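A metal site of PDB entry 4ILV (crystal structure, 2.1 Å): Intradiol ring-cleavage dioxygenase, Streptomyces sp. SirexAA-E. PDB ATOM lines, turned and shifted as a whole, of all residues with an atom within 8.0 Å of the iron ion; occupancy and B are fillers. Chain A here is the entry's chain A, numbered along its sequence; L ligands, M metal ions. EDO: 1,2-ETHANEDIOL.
The backbone carbonyl oxygen (O) of Thr 128 lies within hydrogen-bond range of a ring nitrogen (ND1) of His 130, at 2.9 Å. A ring nitrogen (NE2) of His 130 sits close to the guanidinium group (NH1) of Arg 127 (3.3 Å). The backbone carbonyl oxygen (O) of Trp 87 sits at hydrogen-bond distance from the backbone NH (N) of His 132, 2.8 Å away.
The iron ion is bound by the side-chain hydroxyl of Tyr 95 (2.0 Å), the side-chain hydroxyl of Tyr 124 (2.1 Å), a ring nitrogen (NE2) of His 130 (2.2 Å), a ring nitrogen (NE2) of His 132 (2.3 Å), an oxygen (O2) of the ligand (2.4 Å) and an oxygen (O1) of the ligand (2.4 Å).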
ATOM      1  N   MET A  40     -28.832   4.500 -17.900  1.00  0.00           N
ATOM      2  CA  MET A  40     -29.739   4.015 -18.925  1.00  0.00           C
ATOM      3  C   MET A  40     -29.339   2.662 -19.532  1.00  0.00           C
ATOM      4  O   MET A  40     -28.176   2.255 -19.505  1.00  0.00           O
ATOM      5  CB  MET A  40     -29.955   5.088 -20.003  1.00  0.00           C
ATOM      6  CG  MET A  40     -28.701   5.616 -20.665  1.00  0.00           C
ATOM      7  SD  MET A  40     -29.110   6.871 -21.889  1.00  0.00           S
ATOM      8  CE  MET A  40     -30.054   8.019 -20.889  1.00  0.00           C
ATOM      9  N   GLU A  41     -30.346   1.961 -20.031  1.00  0.00           N
ATOM     10  CA  GLU A  41     -30.184   0.648 -20.644  1.00  0.00           C
ATOM     11  C   GLU A  41     -29.467   0.730 -21.996  1.00  0.00           C
ATOM     12  O   GLU A  41     -28.569  -0.065 -22.276  1.00  0.00           O
ATOM     13  CB  GLU A  41     -31.563   0.023 -20.823  1.00  0.00           C
ATOM     14  CG  GLU A  41     -31.600  -1.337 -21.492  1.00  0.00           C
ATOM     15  CD  GLU A  41     -33.019  -1.892 -21.541  1.00  0.00           C
ATOM     16  OE1 GLU A  41     -33.502  -2.410 -20.515  1.00  0.00           O
ATOM     17  OE2 GLU A  41     -33.660  -1.780 -22.609  1.00  0.00           O
ATOM     18  N   GLY A  42     -29.863   1.688 -22.816  1.00  0.00           N
ATOM     19  CA  GLY A  42     -29.322   1.819 -24.159  1.00  0.00           C
ATOM     20  C   GLY A  42     -30.130   0.965 -25.134  1.00  0.00           C
ATOM     21  O   GLY A  42     -30.848   0.062 -24.709  1.00  0.00           O
ATOM     22  N   PRO A  43     -30.023   1.273 -26.438  1.00  0.00           N
ATOM     23  CA  PRO A  43     -30.800   0.553 -27.452  1.00  0.00           C
ATOM     24  C   PRO A  43     -30.341  -0.889 -27.657  1.00  0.00           C
ATOM     25  O   PRO A  43     -31.097  -1.681 -28.197  1.00  0.00           O
ATOM     26  CB  PRO A  43     -30.574   1.382 -28.726  1.00  0.00           C
ATOM     27  CG  PRO A  43     -29.271   2.069 -28.505  1.00  0.00           C
ATOM     28  CD  PRO A  43     -29.207   2.353 -27.028  1.00  0.00           C
ATOM     29  N   TYR A  44     -29.138  -1.225 -27.194  1.00  0.00           N
ATOM     30  CA  TYR A  44     -28.507  -2.509 -27.547  1.00  0.00           C
ATOM     31  C   TYR A  44     -28.703  -3.658 -26.561  1.00  0.00           C
ATOM     32  O   TYR A  44     -28.046  -4.698 -26.666  1.00  0.00           O
ATOM     33  CB  TYR A  44     -27.031  -2.294 -27.878  1.00  0.00           C
ATOM     34  CG  TYR A  44     -26.848  -1.262 -28.968  1.00  0.00           C
ATOM     35  CD1 TYR A  44     -27.660  -1.275 -30.101  1.00  0.00           C
ATOM     36  CD2 TYR A  44     -25.906  -0.251 -28.850  1.00  0.00           C
ATOM     37  CE1 TYR A  44     -27.521  -0.326 -31.094  1.00  0.00           C
ATOM     38  CE2 TYR A  44     -25.748   0.711 -29.845  1.00  0.00           C
ATOM     39  CZ  TYR A  44     -26.564   0.668 -30.956  1.00  0.00           C
ATOM     40  OH  TYR A  44     -26.416   1.619 -31.950  1.00  0.00           O
ATOM     41  N   PHE A  45     -29.588  -3.482 -25.582  1.00  0.00           N
ATOM     42  CA  PHE A  45     -29.927  -4.592 -24.700  1.00  0.00           C
ATOM     43  C   PHE A  45     -30.807  -5.617 -25.422  1.00  0.00           C
ATOM     44  O   PHE A  45     -31.652  -5.270 -26.238  1.00  0.00           O
ATOM     45  CB  PHE A  45     -30.641  -4.091 -23.434  1.00  0.00           C
ATOM     46  CG  PHE A  45     -31.131  -5.200 -22.543  1.00  0.00           C
ATOM     47  CD1 PHE A  45     -30.240  -5.957 -21.802  1.00  0.00           C
ATOM     48  CD2 PHE A  45     -32.492  -5.489 -22.446  1.00  0.00           C
ATOM     49  CE1 PHE A  45     -30.693  -6.983 -20.966  1.00  0.00           C
ATOM     50  CE2 PHE A  45     -32.946  -6.515 -21.621  1.00  0.00           C
ATOM     51  CZ  PHE A  45     -32.046  -7.262 -20.881  1.00  0.00           C
ATOM     52  N   TRP A  87     -23.898  -7.115 -20.776  1.00  0.00           N
ATOM     53  CA  TRP A  87     -23.739  -7.057 -22.222  1.00  0.00           C
ATOM     54  C   TRP A  87     -22.775  -5.920 -22.603  1.00  0.00           C
ATOM     55  O   TRP A  87     -22.562  -5.007 -21.804  1.00  0.00           O
ATOM     56  CB  TRP A  87     -25.091  -6.983 -22.965  1.00  0.00           C
ATOM     57  CG  TRP A  87     -25.810  -5.677 -22.838  1.00  0.00           C
ATOM     58  CD1 TRP A  87     -25.914  -4.707 -23.798  1.00  0.00           C
ATOM     59  CD2 TRP A  87     -26.552  -5.195 -21.711  1.00  0.00           C
ATOM     60  NE1 TRP A  87     -26.660  -3.654 -23.337  1.00  0.00           N
ATOM     61  CE2 TRP A  87     -27.065  -3.931 -22.057  1.00  0.00           C
ATOM     62  CE3 TRP A  87     -26.807  -5.705 -20.429  1.00  0.00           C
ATOM     63  CZ2 TRP A  87     -27.828  -3.158 -21.171  1.00  0.00           C
ATOM     64  CZ3 TRP A  87     -27.570  -4.942 -19.554  1.00  0.00           C
ATOM     65  CH2 TRP A  87     -28.073  -3.688 -19.929  1.00  0.00           C
ATOM     66  N   GLN A  88     -22.178  -5.999 -23.789  1.00  0.00           N
ATOM     67  CA  GLN A  88     -21.106  -5.070 -24.167  1.00  0.00           C
ATOM     68  C   GLN A  88     -20.765  -5.192 -25.637  1.00  0.00           C
ATOM     69  O   GLN A  88     -21.143  -6.161 -26.282  1.00  0.00           O
ATOM     70  CB  GLN A  88     -19.832  -5.395 -23.388  1.00  0.00           C
ATOM     71  CG  GLN A  88     -19.219  -6.745 -23.817  1.00  0.00           C
ATOM     72  CD  GLN A  88     -17.839  -6.984 -23.250  1.00  0.00           C
ATOM     73  OE1 GLN A  88     -17.686  -7.437 -22.106  1.00  0.00           O
ATOM     74  NE2 GLN A  88     -16.817  -6.692 -24.038  1.00  0.00           N
ATOM     75  N   ALA A  89     -20.021  -4.218 -26.137  1.00  0.00           N
ATOM     76  CA  ALA A  89     -19.529  -4.287 -27.518  1.00  0.00           C
ATOM     77  C   ALA A  89     -18.329  -5.218 -27.600  1.00  0.00           C
ATOM     78  O   ALA A  89     -17.654  -5.469 -26.588  1.00  0.00           O
ATOM     79  CB  ALA A  89     -19.149  -2.896 -28.014  1.00  0.00           C
ATOM     80  N   GLY A  93     -16.137  -2.601 -31.201  1.00  0.00           N
ATOM     81  CA  GLY A  93     -17.196  -1.683 -30.835  1.00  0.00           C
ATOM     82  C   GLY A  93     -18.578  -2.048 -31.336  1.00  0.00           C
ATOM     83  O   GLY A  93     -19.501  -1.233 -31.245  1.00  0.00           O
ATOM     84  N   TYR A  95     -22.150  -4.259 -31.169  1.00  0.00           N
ATOM     85  CA  TYR A  95     -23.020  -5.115 -30.356  1.00  0.00           C
ATOM     86  C   TYR A  95     -23.670  -6.149 -31.273  1.00  0.00           C
ATOM     87  O   TYR A  95     -23.954  -5.875 -32.441  1.00  0.00           O
ATOM     88  CB  TYR A  95     -24.122  -4.311 -29.652  1.00  0.00           C
ATOM     89  CG  TYR A  95     -23.644  -3.413 -28.527  1.00  0.00           C
ATOM     90  CD1 TYR A  95     -23.704  -3.836 -27.201  1.00  0.00           C
ATOM     91  CD2 TYR A  95     -23.143  -2.139 -28.795  1.00  0.00           C
ATOM     92  CE1 TYR A  95     -23.262  -3.015 -26.162  1.00  0.00           C
ATOM     93  CE2 TYR A  95     -22.702  -1.309 -27.756  1.00  0.00           C
ATOM     94  CZ  TYR A  95     -22.759  -1.762 -26.439  1.00  0.00           C
ATOM     95  OH  TYR A  95     -22.326  -0.953 -25.408  1.00  0.00           O
ATOM     96  N   GLY A 122     -14.595  -2.436 -27.321  1.00  0.00           N
ATOM     97  CA  GLY A 122     -14.096  -1.396 -28.190  1.00  0.00           C
ATOM     98  C   GLY A 122     -14.945  -0.129 -28.124  1.00  0.00           C
ATOM     99  O   GLY A 122     -16.094  -0.157 -27.681  1.00  0.00           O
ATOM    100  N   TYR A 124     -17.089   3.032 -29.697  1.00  0.00           N
ATOM    101  CA  TYR A 124     -18.022   3.298 -30.785  1.00  0.00           C
ATOM    102  C   TYR A 124     -18.500   4.753 -30.700  1.00  0.00           C
ATOM    103  O   TYR A 124     -18.158   5.447 -29.739  1.00  0.00           O
ATOM    104  CB  TYR A 124     -19.167   2.266 -30.779  1.00  0.00           C
ATOM    105  CG  TYR A 124     -20.072   2.236 -29.569  1.00  0.00           C
ATOM    106  CD1 TYR A 124     -21.171   3.089 -29.479  1.00  0.00           C
ATOM    107  CD2 TYR A 124     -19.869   1.320 -28.548  1.00  0.00           C
ATOM    108  CE1 TYR A 124     -22.023   3.051 -28.392  1.00  0.00           C
ATOM    109  CE2 TYR A 124     -20.720   1.284 -27.441  1.00  0.00           C
ATOM    110  CZ  TYR A 124     -21.801   2.138 -27.373  1.00  0.00           C
ATOM    111  OH  TYR A 124     -22.654   2.110 -26.296  1.00  0.00           O
ATOM    112  N   ARG A 127     -19.474   7.497 -27.332  1.00  0.00           N
ATOM    113  CA  ARG A 127     -19.426   6.948 -25.977  1.00  0.00           C
ATOM    114  C   ARG A 127     -18.009   6.588 -25.547  1.00  0.00           C
ATOM    115  O   ARG A 127     -17.205   6.105 -26.347  1.00  0.00           O
ATOM    116  CB  ARG A 127     -20.313   5.700 -25.857  1.00  0.00           C
ATOM    117  CG  ARG A 127     -21.785   5.916 -26.177  1.00  0.00           C
ATOM    118  CD  ARG A 127     -22.705   5.661 -24.996  1.00  0.00           C
ATOM    119  NE  ARG A 127     -22.102   6.046 -23.727  1.00  0.00           N
ATOM    120  CZ  ARG A 127     -22.210   5.317 -22.615  1.00  0.00           C
ATOM    121  NH1 ARG A 127     -22.898   4.180 -22.632  1.00  0.00           N
ATOM    122  NH2 ARG A 127     -21.630   5.724 -21.485  1.00  0.00           N
ATOM    123  N   THR A 128     -17.747   6.789 -24.268  1.00  0.00           N
ATOM    124  CA  THR A 128     -16.530   6.259 -23.667  1.00  0.00           C
ATOM    125  C   THR A 128     -16.675   4.743 -23.521  1.00  0.00           C
ATOM    126  O   THR A 128     -17.735   4.185 -23.792  1.00  0.00           O
ATOM    127  CB  THR A 128     -16.246   6.899 -22.309  1.00  0.00           C
ATOM    128  OG1 THR A 128     -14.905   6.569 -21.905  1.00  0.00           O
ATOM    129  CG2 THR A 128     -17.237   6.408 -21.274  1.00  0.00           C
ATOM    130  N   ARG A 129     -15.597   4.087 -23.107  1.00  0.00           N
ATOM    131  CA  ARG A 129     -15.600   2.629 -22.992  1.00  0.00           C
ATOM    132  C   ARG A 129     -16.452   2.172 -21.786  1.00  0.00           C
ATOM    133  O   ARG A 129     -16.347   2.730 -20.684  1.00  0.00           O
ATOM    134  CB  ARG A 129     -14.168   2.149 -22.848  1.00  0.00           C
ATOM    135  CG  ARG A 129     -13.971   0.736 -23.288  1.00  0.00           C
ATOM    136  CD  ARG A 129     -12.534   0.298 -23.147  1.00  0.00           C
ATOM    137  NE  ARG A 129     -11.603   1.272 -23.718  1.00  0.00           N
ATOM    138  CZ  ARG A 129     -11.228   1.313 -24.987  1.00  0.00           C
ATOM    139  NH1 ARG A 129     -11.705   0.444 -25.882  1.00  0.00           N
ATOM    140  NH2 ARG A 129     -10.359   2.247 -25.362  1.00  0.00           N
ATOM    141  N   HIS A 130     -17.275   1.133 -21.970  1.00  0.00           N
ATOM    142  CA  HIS A 130     -18.166   0.676 -20.892  1.00  0.00           C
ATOM    143  C   HIS A 130     -18.647  -0.753 -21.070  1.00  0.00           C
ATOM    144  O   HIS A 130     -18.697  -1.273 -22.177  1.00  0.00           O
ATOM    145  CB  HIS A 130     -19.403   1.583 -20.796  1.00  0.00           C
ATOM    146  CG  HIS A 130     -20.218   1.605 -22.061  1.00  0.00           C
ATOM    147  ND1 HIS A 130     -19.843   2.297 -23.178  1.00  0.00           N
ATOM    148  CD2 HIS A 130     -21.384   0.982 -22.373  1.00  0.00           C
ATOM    149  CE1 HIS A 130     -20.734   2.119 -24.138  1.00  0.00           C
ATOM    150  NE2 HIS A 130     -21.684   1.320 -23.673  1.00  0.00           N
ATOM    151  N   ILE A 131     -19.064  -1.360 -19.964  1.00  0.00           N
ATOM    152  CA  ILE A 131     -19.765  -2.639 -19.985  1.00  0.00           C
ATOM    153  C   ILE A 131     -21.130  -2.435 -19.338  1.00  0.00           C
ATOM    154  O   ILE A 131     -21.234  -1.834 -18.266  1.00  0.00           O
ATOM    155  CB  ILE A 131     -18.984  -3.691 -19.164  1.00  0.00           C
ATOM    156  CG1 ILE A 131     -17.683  -4.057 -19.879  1.00  0.00           C
ATOM    157  CG2 ILE A 131     -19.835  -4.930 -18.936  1.00  0.00           C
ATOM    158  CD1 ILE A 131     -16.777  -4.960 -19.032  1.00  0.00           C
ATOM    159  N   HIS A 132     -22.194  -2.916 -19.984  1.00  0.00           N
ATOM    160  CA  HIS A 132     -23.519  -2.761 -19.418  1.00  0.00           C
ATOM    161  C   HIS A 132     -23.849  -3.876 -18.425  1.00  0.00           C
ATOM    162  O   HIS A 132     -23.419  -5.008 -18.612  1.00  0.00           O
ATOM    163  CB  HIS A 132     -24.580  -2.774 -20.515  1.00  0.00           C
ATOM    164  CG  HIS A 132     -24.545  -1.603 -21.432  1.00  0.00           C
ATOM    165  ND1 HIS A 132     -25.238  -0.440 -21.180  1.00  0.00           N
ATOM    166  CD2 HIS A 132     -23.931  -1.418 -22.631  1.00  0.00           C
ATOM    167  CE1 HIS A 132     -25.036   0.417 -22.163  1.00  0.00           C
ATOM    168  NE2 HIS A 132     -24.237  -0.150 -23.050  1.00  0.00           N
ATOM    169  N   GLN A 146     -24.000   0.867 -15.658  1.00  0.00           N
ATOM    170  CA  GLN A 146     -22.833   0.610 -16.501  1.00  0.00           C
ATOM    171  C   GLN A 146     -21.531   0.643 -15.690  1.00  0.00           C
ATOM    172  O   GLN A 146     -21.475   1.254 -14.627  1.00  0.00           O
ATOM    173  CB  GLN A 146     -22.744   1.661 -17.596  1.00  0.00           C
ATOM    174  CG  GLN A 146     -23.973   1.735 -18.466  1.00  0.00           C
ATOM    175  CD  GLN A 146     -23.864   2.799 -19.543  1.00  0.00           C
ATOM    176  OE1 GLN A 146     -22.763   3.134 -19.987  1.00  0.00           O
ATOM    177  NE2 GLN A 146     -25.007   3.325 -19.968  1.00  0.00           N
ATOM    178  N   LEU A 160     -22.291  10.970 -19.982  1.00  0.00           N
ATOM    179  CA  LEU A 160     -22.894   9.883 -19.235  1.00  0.00           C
ATOM    180  C   LEU A 160     -21.933   9.296 -18.195  1.00  0.00           C
ATOM    181  O   LEU A 160     -22.350   8.590 -17.286  1.00  0.00           O
ATOM    182  CB  LEU A 160     -23.333   8.764 -20.172  1.00  0.00           C
ATOM    183  CG  LEU A 160     -24.804   8.684 -20.579  1.00  0.00           C
ATOM    184  CD1 LEU A 160     -25.171   9.845 -21.491  1.00  0.00           C
ATOM    185  CD2 LEU A 160     -25.079   7.353 -21.265  1.00  0.00           C
HETATM  186  C1  EDO L   1     -25.508   3.188 -25.286  1.00  0.00           C
HETATM  187  O1  EDO L   1     -24.457   2.779 -24.380  1.00  0.00           O
HETATM  188  C2  EDO L   1     -25.634   2.191 -26.448  1.00  0.00           C
HETATM  189  O2  EDO L   1     -25.465   0.838 -25.977  1.00  0.00           O
HETATM  190 FE    FE M   1     -23.343   0.752 -24.920  1.00  0.00          FE
